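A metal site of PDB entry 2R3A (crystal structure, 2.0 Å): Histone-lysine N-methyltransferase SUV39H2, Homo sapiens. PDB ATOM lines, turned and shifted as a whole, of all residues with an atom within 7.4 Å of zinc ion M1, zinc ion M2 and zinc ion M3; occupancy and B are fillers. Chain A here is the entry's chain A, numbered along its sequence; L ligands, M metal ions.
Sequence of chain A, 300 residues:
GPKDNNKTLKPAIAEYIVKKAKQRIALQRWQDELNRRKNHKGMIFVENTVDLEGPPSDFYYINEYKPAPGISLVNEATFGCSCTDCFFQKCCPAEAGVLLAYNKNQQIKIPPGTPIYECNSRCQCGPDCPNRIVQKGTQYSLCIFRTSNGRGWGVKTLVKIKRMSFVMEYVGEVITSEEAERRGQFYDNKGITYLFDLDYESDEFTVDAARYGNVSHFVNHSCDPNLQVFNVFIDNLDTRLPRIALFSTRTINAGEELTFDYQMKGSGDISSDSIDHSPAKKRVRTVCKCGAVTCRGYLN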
ATOM      1  N   PHE A  79      12.792  34.560  27.785  1.00  0.00           N
ATOM      2  CA  PHE A  79      13.147  33.427  28.629  1.00  0.00           C
ATOM      3  C   PHE A  79      13.539  32.252  27.714  1.00  0.00           C
ATOM      4  O   PHE A  79      12.969  32.057  26.620  1.00  0.00           O
ATOM      5  CB  PHE A  79      11.978  32.996  29.539  1.00  0.00           C
ATOM      6  CG  PHE A  79      11.377  34.119  30.368  1.00  0.00           C
ATOM      7  CD1 PHE A  79      11.998  34.548  31.537  1.00  0.00           C
ATOM      8  CD2 PHE A  79      10.158  34.704  30.005  1.00  0.00           C
ATOM      9  CE1 PHE A  79      11.426  35.560  32.325  1.00  0.00           C
ATOM     10  CE2 PHE A  79       9.593  35.710  30.797  1.00  0.00           C
ATOM     11  CZ  PHE A  79      10.226  36.129  31.958  1.00  0.00           C
ATOM     12  N   GLY A  80      14.525  31.486  28.160  1.00  0.00           N
ATOM     13  CA  GLY A  80      14.867  30.252  27.505  1.00  0.00           C
ATOM     14  C   GLY A  80      14.721  29.118  28.489  1.00  0.00           C
ATOM     15  O   GLY A  80      14.265  29.307  29.620  1.00  0.00           O
ATOM     16  N   CYS A  81      15.127  27.938  28.020  1.00  0.00           N
ATOM     17  CA  CYS A  81      15.199  26.718  28.815  1.00  0.00           C
ATOM     18  C   CYS A  81      16.538  26.664  29.570  1.00  0.00           C
ATOM     19  O   CYS A  81      17.429  27.464  29.291  1.00  0.00           O
ATOM     20  CB  CYS A  81      15.110  25.522  27.846  1.00  0.00           C
ATOM     21  SG  CYS A  81      16.578  25.306  26.767  1.00  0.00           S
ATOM     22  N   SER A  82      16.692  25.683  30.469  1.00  0.00           N
ATOM     23  CA  SER A  82      17.931  25.488  31.240  1.00  0.00           C
ATOM     24  C   SER A  82      18.518  24.088  31.145  1.00  0.00           C
ATOM     25  O   SER A  82      19.448  23.757  31.945  1.00  0.00           O
ATOM     26  CB  SER A  82      17.735  25.804  32.735  1.00  0.00           C
ATOM     27  OG  SER A  82      16.592  26.574  32.973  1.00  0.00           O
ATOM     28  N   CYS A  83      17.979  23.276  30.220  1.00  0.00           N
ATOM     29  CA  CYS A  83      18.478  21.955  29.891  1.00  0.00           C
ATOM     30  C   CYS A  83      19.974  21.889  29.749  1.00  0.00           C
ATOM     31  O   CYS A  83      20.611  22.796  29.175  1.00  0.00           O
ATOM     32  CB  CYS A  83      17.832  21.418  28.607  1.00  0.00           C
ATOM     33  SG  CYS A  83      16.092  21.830  28.396  1.00  0.00           S
ATOM     34  N   THR A  84      20.525  20.803  30.284  1.00  0.00           N
ATOM     35  CA  THR A  84      21.865  20.363  29.930  1.00  0.00           C
ATOM     36  C   THR A  84      21.780  19.349  28.762  1.00  0.00           C
ATOM     37  O   THR A  84      22.770  19.085  28.083  1.00  0.00           O
ATOM     38  CB  THR A  84      22.587  19.712  31.102  1.00  0.00           C
ATOM     39  OG1 THR A  84      21.733  18.739  31.716  1.00  0.00           O
ATOM     40  CG2 THR A  84      23.030  20.760  32.160  1.00  0.00           C
ATOM     41  N   ASP A  85      20.590  18.794  28.557  1.00  0.00           N
ATOM     42  CA  ASP A  85      20.287  17.931  27.420  1.00  0.00           C
ATOM     43  C   ASP A  85      18.909  18.318  26.875  1.00  0.00           C
ATOM     44  O   ASP A  85      17.882  17.801  27.321  1.00  0.00           O
ATOM     45  CB  ASP A  85      20.308  16.462  27.848  1.00  0.00           C
ATOM     46  CG  ASP A  85      20.315  15.495  26.657  1.00  0.00           C
ATOM     47  OD1 ASP A  85      20.043  15.898  25.521  1.00  0.00           O
ATOM     48  OD2 ASP A  85      20.606  14.298  26.895  1.00  0.00           O
ATOM     49  N   CYS A  86      18.884  19.272  25.931  1.00  0.00           N
ATOM     50  CA  CYS A  86      17.598  19.753  25.361  1.00  0.00           C
ATOM     51  C   CYS A  86      16.853  18.677  24.590  1.00  0.00           C
ATOM     52  O   CYS A  86      15.633  18.749  24.430  1.00  0.00           O
ATOM     53  CB  CYS A  86      17.835  20.930  24.442  1.00  0.00           C
ATOM     54  SG  CYS A  86      18.265  22.403  25.327  1.00  0.00           S
ATOM     55  N   PHE A  87      17.575  17.681  24.101  1.00  0.00           N
ATOM     56  CA  PHE A  87      16.930  16.576  23.391  1.00  0.00           C
ATOM     57  C   PHE A  87      15.999  15.719  24.302  1.00  0.00           C
ATOM     58  O   PHE A  87      14.954  15.224  23.858  1.00  0.00           O
ATOM     59  CB  PHE A  87      17.967  15.712  22.654  1.00  0.00           C
ATOM     60  CG  PHE A  87      17.352  14.771  21.659  1.00  0.00           C
ATOM     61  CD1 PHE A  87      16.945  15.234  20.398  1.00  0.00           C
ATOM     62  CD2 PHE A  87      17.114  13.427  21.984  1.00  0.00           C
ATOM     63  CE1 PHE A  87      16.324  14.360  19.480  1.00  0.00           C
ATOM     64  CE2 PHE A  87      16.507  12.550  21.066  1.00  0.00           C
ATOM     65  CZ  PHE A  87      16.102  13.021  19.812  1.00  0.00           C
ATOM     66  N   GLN A  89      15.342  16.553  28.009  1.00  0.00           N
ATOM     67  CA  GLN A  89      14.716  17.281  29.130  1.00  0.00           C
ATOM     68  C   GLN A  89      13.533  18.126  28.653  1.00  0.00           C
ATOM     69  O   GLN A  89      13.295  18.241  27.446  1.00  0.00           O
ATOM     70  CB  GLN A  89      15.773  18.126  29.868  1.00  0.00           C
ATOM     71  CG  GLN A  89      16.856  17.262  30.509  1.00  0.00           C
ATOM     72  CD  GLN A  89      17.845  18.075  31.279  1.00  0.00           C
ATOM     73  OE1 GLN A  89      18.318  19.112  30.813  1.00  0.00           O
ATOM     74  NE2 GLN A  89      18.196  17.590  32.502  1.00  0.00           N
ATOM     75  N   LYS A  90      12.790  18.697  29.587  1.00  0.00           N
ATOM     76  CA  LYS A  90      11.646  19.564  29.220  1.00  0.00           C
ATOM     77  C   LYS A  90      12.205  20.902  28.760  1.00  0.00           C
ATOM     78  O   LYS A  90      12.866  21.601  29.528  1.00  0.00           O
ATOM     79  CB  LYS A  90      10.694  19.773  30.400  1.00  0.00           C
ATOM     80  CG  LYS A  90       9.651  18.699  30.581  1.00  0.00           C
ATOM     81  CD  LYS A  90       8.859  18.922  31.864  1.00  0.00           C
ATOM     82  CE  LYS A  90       9.172  17.845  32.916  1.00  0.00           C
ATOM     83  NZ  LYS A  90       8.362  16.627  32.624  1.00  0.00           N
ATOM     84  N   CYS A  91      11.959  21.247  27.505  1.00  0.00           N
ATOM     85  CA  CYS A  91      12.700  22.266  26.804  1.00  0.00           C
ATOM     86  C   CYS A  91      11.727  23.302  26.200  1.00  0.00           C
ATOM     87  O   CYS A  91      10.540  23.299  26.520  1.00  0.00           O
ATOM     88  CB  CYS A  91      13.535  21.567  25.735  1.00  0.00           C
ATOM     89  SG  CYS A  91      14.562  22.582  24.683  1.00  0.00           S
ATOM     90  N   CYS A  92      12.250  24.185  25.355  1.00  0.00           N
ATOM     91  CA  CYS A  92      11.408  25.230  24.755  1.00  0.00           C
ATOM     92  C   CYS A  92      10.111  24.775  24.079  1.00  0.00           C
ATOM     93  O   CYS A  92       9.049  25.384  24.311  1.00  0.00           O
ATOM     94  CB  CYS A  92      12.237  26.130  23.827  1.00  0.00           C
ATOM     95  SG  CYS A  92      13.591  27.077  24.683  1.00  0.00           S
ATOM     96  N   PRO A  93      10.175  23.720  23.222  1.00  0.00           N
ATOM     97  CA  PRO A  93       8.884  23.308  22.642  1.00  0.00           C
ATOM     98  C   PRO A  93       7.847  22.880  23.702  1.00  0.00           C
ATOM     99  O   PRO A  93       6.686  23.273  23.617  1.00  0.00           O
ATOM    100  CB  PRO A  93       9.244  22.118  21.708  1.00  0.00           C
ATOM    101  CG  PRO A  93      10.706  22.103  21.594  1.00  0.00           C
ATOM    102  CD  PRO A  93      11.275  22.865  22.768  1.00  0.00           C
ATOM    103  N   TYR A 117       9.587  25.621  17.684  1.00  0.00           N
ATOM    104  CA  TYR A 117      10.097  26.510  18.737  1.00  0.00           C
ATOM    105  C   TYR A 117      11.509  26.041  19.005  1.00  0.00           C
ATOM    106  O   TYR A 117      11.730  25.000  19.655  1.00  0.00           O
ATOM    107  CB  TYR A 117       9.238  26.461  20.027  1.00  0.00           C
ATOM    108  CG  TYR A 117       7.955  27.253  19.914  1.00  0.00           C
ATOM    109  CD1 TYR A 117       7.889  28.589  20.357  1.00  0.00           C
ATOM    110  CD2 TYR A 117       6.812  26.681  19.369  1.00  0.00           C
ATOM    111  CE1 TYR A 117       6.736  29.310  20.226  1.00  0.00           C
ATOM    112  CE2 TYR A 117       5.631  27.411  19.223  1.00  0.00           C
ATOM    113  CZ  TYR A 117       5.604  28.723  19.665  1.00  0.00           C
ATOM    114  OH  TYR A 117       4.438  29.476  19.576  1.00  0.00           O
ATOM    115  N   GLU A 118      12.475  26.758  18.454  1.00  0.00           N
ATOM    116  CA  GLU A 118      13.889  26.413  18.647  1.00  0.00           C
ATOM    117  C   GLU A 118      14.400  27.093  19.923  1.00  0.00           C
ATOM    118  O   GLU A 118      13.779  28.046  20.430  1.00  0.00           O
ATOM    119  CB  GLU A 118      14.774  26.877  17.476  1.00  0.00           C
ATOM    120  CG  GLU A 118      14.389  26.254  16.119  1.00  0.00           C
ATOM    121  CD  GLU A 118      15.550  26.186  15.150  1.00  0.00           C
ATOM    122  OE1 GLU A 118      16.525  26.959  15.252  1.00  0.00           O
ATOM    123  OE2 GLU A 118      15.508  25.333  14.236  1.00  0.00           O
ATOM    124  N   CYS A 119      15.543  26.642  20.427  1.00  0.00           N
ATOM    125  CA  CYS A 119      16.179  27.323  21.523  1.00  0.00           C
ATOM    126  C   CYS A 119      16.741  28.658  21.009  1.00  0.00           C
ATOM    127  O   CYS A 119      16.944  28.839  19.796  1.00  0.00           O
ATOM    128  CB  CYS A 119      17.295  26.459  22.115  1.00  0.00           C
ATOM    129  SG  CYS A 119      16.677  25.013  22.939  1.00  0.00           S
ATOM    130  N   ASN A 120      16.976  29.588  21.932  1.00  0.00           N
ATOM    131  CA  ASN A 120      17.190  30.981  21.552  1.00  0.00           C
ATOM    132  C   ASN A 120      18.346  31.578  22.362  1.00  0.00           C
ATOM    133  O   ASN A 120      19.055  30.817  23.058  1.00  0.00           O
ATOM    134  CB  ASN A 120      15.885  31.766  21.686  1.00  0.00           C
ATOM    135  CG  ASN A 120      15.334  31.785  23.121  1.00  0.00           C
ATOM    136  OD1 ASN A 120      15.963  32.316  24.040  1.00  0.00           O
ATOM    137  ND2 ASN A 120      14.161  31.223  23.310  1.00  0.00           N
ATOM    138  N   ARG A 122      18.475  33.268  24.914  1.00  0.00           N
ATOM    139  CA  ARG A 122      18.262  33.198  26.344  1.00  0.00           C
ATOM    140  C   ARG A 122      18.405  31.804  26.925  1.00  0.00           C
ATOM    141  O   ARG A 122      18.468  31.670  28.133  1.00  0.00           O
ATOM    142  CB  ARG A 122      16.890  33.793  26.713  1.00  0.00           C
ATOM    143  N   CYS A 123      18.427  30.742  26.097  1.00  0.00           N
ATOM    144  CA  CYS A 123      18.609  29.381  26.624  1.00  0.00           C
ATOM    145  C   CYS A 123      20.061  29.174  27.068  1.00  0.00           C
ATOM    146  O   CYS A 123      20.968  29.827  26.535  1.00  0.00           O
ATOM    147  CB  CYS A 123      18.266  28.334  25.557  1.00  0.00           C
ATOM    148  SG  CYS A 123      16.588  28.512  24.926  1.00  0.00           S
ATOM    149  N   GLN A 124      20.275  28.241  27.992  1.00  0.00           N
ATOM    150  CA  GLN A 124      21.614  27.932  28.501  1.00  0.00           C
ATOM    151  C   GLN A 124      22.487  27.164  27.530  1.00  0.00           C
ATOM    152  O   GLN A 124      23.736  27.208  27.629  1.00  0.00           O
ATOM    153  CB  GLN A 124      21.546  27.142  29.811  1.00  0.00           C
ATOM    154  CG  GLN A 124      21.005  27.895  31.070  1.00  0.00           C
ATOM    155  CD  GLN A 124      21.803  29.152  31.411  1.00  0.00           C
ATOM    156  OE1 GLN A 124      23.026  29.106  31.670  1.00  0.00           O
ATOM    157  NE2 GLN A 124      21.129  30.285  31.413  1.00  0.00           N
ATOM    158  N   CYS A 125      21.829  26.413  26.615  1.00  0.00           N
ATOM    159  CA  CYS A 125      22.510  25.511  25.687  1.00  0.00           C
ATOM    160  C   CYS A 125      23.327  26.254  24.645  1.00  0.00           C
ATOM    161  O   CYS A 125      23.010  27.386  24.264  1.00  0.00           O
ATOM    162  CB  CYS A 125      21.496  24.605  24.982  1.00  0.00           C
ATOM    163  SG  CYS A 125      20.203  25.563  24.078  1.00  0.00           S
ATOM    164  N   GLY A 126      24.364  25.588  24.166  1.00  0.00           N
ATOM    165  CA  GLY A 126      25.243  26.135  23.141  1.00  0.00           C
ATOM    166  C   GLY A 126      24.757  25.785  21.730  1.00  0.00           C
ATOM    167  O   GLY A 126      23.686  25.199  21.557  1.00  0.00           O
ATOM    168  N   ASP A 128      25.480  23.588  19.438  1.00  0.00           N
ATOM    169  CA  ASP A 128      25.254  22.231  18.982  1.00  0.00           C
ATOM    170  C   ASP A 128      24.058  21.553  19.672  1.00  0.00           C
ATOM    171  O   ASP A 128      23.857  20.339  19.563  1.00  0.00           O
ATOM    172  CB  ASP A 128      26.583  21.446  18.995  1.00  0.00           C
ATOM    173  CG  ASP A 128      27.713  22.141  18.151  1.00  0.00           C
ATOM    174  OD1 ASP A 128      27.431  22.799  17.097  1.00  0.00           O
ATOM    175  OD2 ASP A 128      28.903  22.015  18.549  1.00  0.00           O
ATOM    176  N   CYS A 129      23.214  22.352  20.331  1.00  0.00           N
ATOM    177  CA  CYS A 129      21.888  21.907  20.748  1.00  0.00           C
ATOM    178  C   CYS A 129      21.078  21.348  19.535  1.00  0.00           C
ATOM    179  O   CYS A 129      20.972  21.989  18.471  1.00  0.00           O
ATOM    180  CB  CYS A 129      21.113  23.038  21.413  1.00  0.00           C
ATOM    181  SG  CYS A 129      19.373  22.647  21.718  1.00  0.00           S
ATOM    182  N   PRO A 130      20.507  20.138  19.697  1.00  0.00           N
ATOM    183  CA  PRO A 130      19.781  19.524  18.600  1.00  0.00           C
ATOM    184  C   PRO A 130      18.516  20.325  18.294  1.00  0.00           C
ATOM    185  O   PRO A 130      17.836  20.025  17.324  1.00  0.00           O
ATOM    186  CB  PRO A 130      19.409  18.142  19.158  1.00  0.00           C
ATOM    187  CG  PRO A 130      19.334  18.377  20.634  1.00  0.00           C
ATOM    188  CD  PRO A 130      20.484  19.272  20.902  1.00  0.00           C
ATOM    189  N   ASN A 131      18.180  21.301  19.162  1.00  0.00           N
ATOM    190  CA  ASN A 131      17.026  22.197  18.895  1.00  0.00           C
ATOM    191  C   ASN A 131      17.435  23.555  18.296  1.00  0.00           C
ATOM    192  O   ASN A 131      16.723  24.544  18.400  1.00  0.00           O
ATOM    193  CB  ASN A 131      16.090  22.273  20.112  1.00  0.00           C
ATOM    194  CG  ASN A 131      14.742  22.964  19.816  1.00  0.00           C
ATOM    195  OD1 ASN A 131      14.148  23.573  20.723  1.00  0.00           O
ATOM    196  ND2 ASN A 131      14.247  22.829  18.608  1.00  0.00           N
ATOM    197  N   ARG A 132      18.578  23.600  17.627  1.00  0.00           N
ATOM    198  CA  ARG A 132      19.006  24.843  16.952  1.00  0.00           C
ATOM    199  C   ARG A 132      19.401  24.488  15.518  1.00  0.00           C
ATOM    200  O   ARG A 132      20.561  24.184  15.256  1.00  0.00           O
ATOM    201  CB  ARG A 132      20.204  25.454  17.698  1.00  0.00           C
ATOM    202  CG  ARG A 132      19.906  26.000  19.125  1.00  0.00           C
ATOM    203  CD  ARG A 132      21.239  26.415  19.804  1.00  0.00           C
ATOM    204  NE  ARG A 132      21.096  26.973  21.158  1.00  0.00           N
ATOM    205  CZ  ARG A 132      20.716  28.210  21.443  1.00  0.00           C
ATOM    206  NH1 ARG A 132      20.403  29.076  20.479  1.00  0.00           N
ATOM    207  NH2 ARG A 132      20.662  28.604  22.709  1.00  0.00           N
HETATM  208  N1  LIG L   1      23.577  19.192  23.295  1.00  0.00           N
HETATM  209  C1  LIG L   1      23.301  20.603  23.741  1.00  0.00           C
HETATM  210  C2  LIG L   1      24.548  21.468  24.030  1.00  0.00           C
HETATM  211  O1  LIG L   1      25.563  21.381  23.291  1.00  0.00           O
HETATM  212  C3  LIG L   1      22.285  20.606  24.905  1.00  0.00           C
HETATM  213  O2  LIG L   1      21.121  19.881  24.535  1.00  0.00           O
HETATM  214  O3  LIG L   1      24.568  22.305  24.976  1.00  0.00           O
HETATM  215 ZN    ZN M   1      18.676  23.949  23.593  1.00  0.00          ZN
HETATM  216 ZN    ZN M   2      16.326  22.972  26.303  1.00  0.00          ZN
HETATM  217 ZN    ZN M   3      15.734  26.328  24.760  1.00  0.00          ZN
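Five residues have an atom within 4 Å of zinc ion M2: Cys 81, Cys 83, Cys 86, Cys 91 and Cys 119. The nearest printed residue that does not touch zinc ion M2 is Cys 92 (4.4 Å).
Five residues have an atom within 4 Å of zinc ion M3: Cys 81, Cys 91, Cys 92, Cys 119 and Cys 123.
The guanidinium group of Arg 132 lies within hydrogen-bond range of the backbone carbonyl oxygen of Cys 125. The backbone NH (N) of Asn 120 lies close to the side-chain sulfur (SG) of Cys 123 (3.2 Å). N of Cys 119 lies within hydrogen-bond range of O of Asn 131 (3.1 Å). N of Asn 131 lies close to SG of Cys 129 (3.1 Å). The backbone NH (N) of Gln 124 sits at hydrogen-bond distance from the backbone carbonyl oxygen (O) of Cys 81, 3.2 Å away. The side-chain sulfur (SG) of Cys 83 sits close to the backbone carbonyl oxygen (O) of Lys 90 (3.4 Å).
N of Cys 86 is in hydrogen-bond range of O2 of the ligand (2.7 Å). N of Gly 126 lies within hydrogen-bond range of O3 of the ligand (3.4 Å).
Zinc ion M1 is bound by the side-chain sulfur (SG) of Cys 125 (2.3 Å), the side-chain sulfur (SG) of Cys 119 (2.4 Å), the side-chain sulfur (SG) of Cys 86 (2.4 Å) and the side-chain sulfur (SG) of Cys 129 (2.4 Å). Zinc ion M1 has four donor atoms within binding distance.
Along chain A the residues within 4 Å of zinc ion M1 span positions 86 to 129. The nearest printed residue that does not touch zinc ion M1 is Cys 81 (4.04 Å).
Zinc ion M2 is bound by the side-chain sulfur (SG) of Cys 86 (2.2 Å), the side-chain sulfur (SG) of Cys 81 (2.4 Å), the side-chain sulfur (SG) of Cys 83 (2.4 Å) and the side-chain sulfur (SG) of Cys 91 (2.4 Å). Zinc ion M2 has four donor atoms within binding distance.
Zinc ion M3 is bound by the side-chain sulfur of Cys 92 (2.3 Å), the side-chain sulfur of Cys 123 (2.4 Å), the side-chain sulfur of Cys 81 (2.4 Å) and the side-chain sulfur of Cys 119 (2.4 Å).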
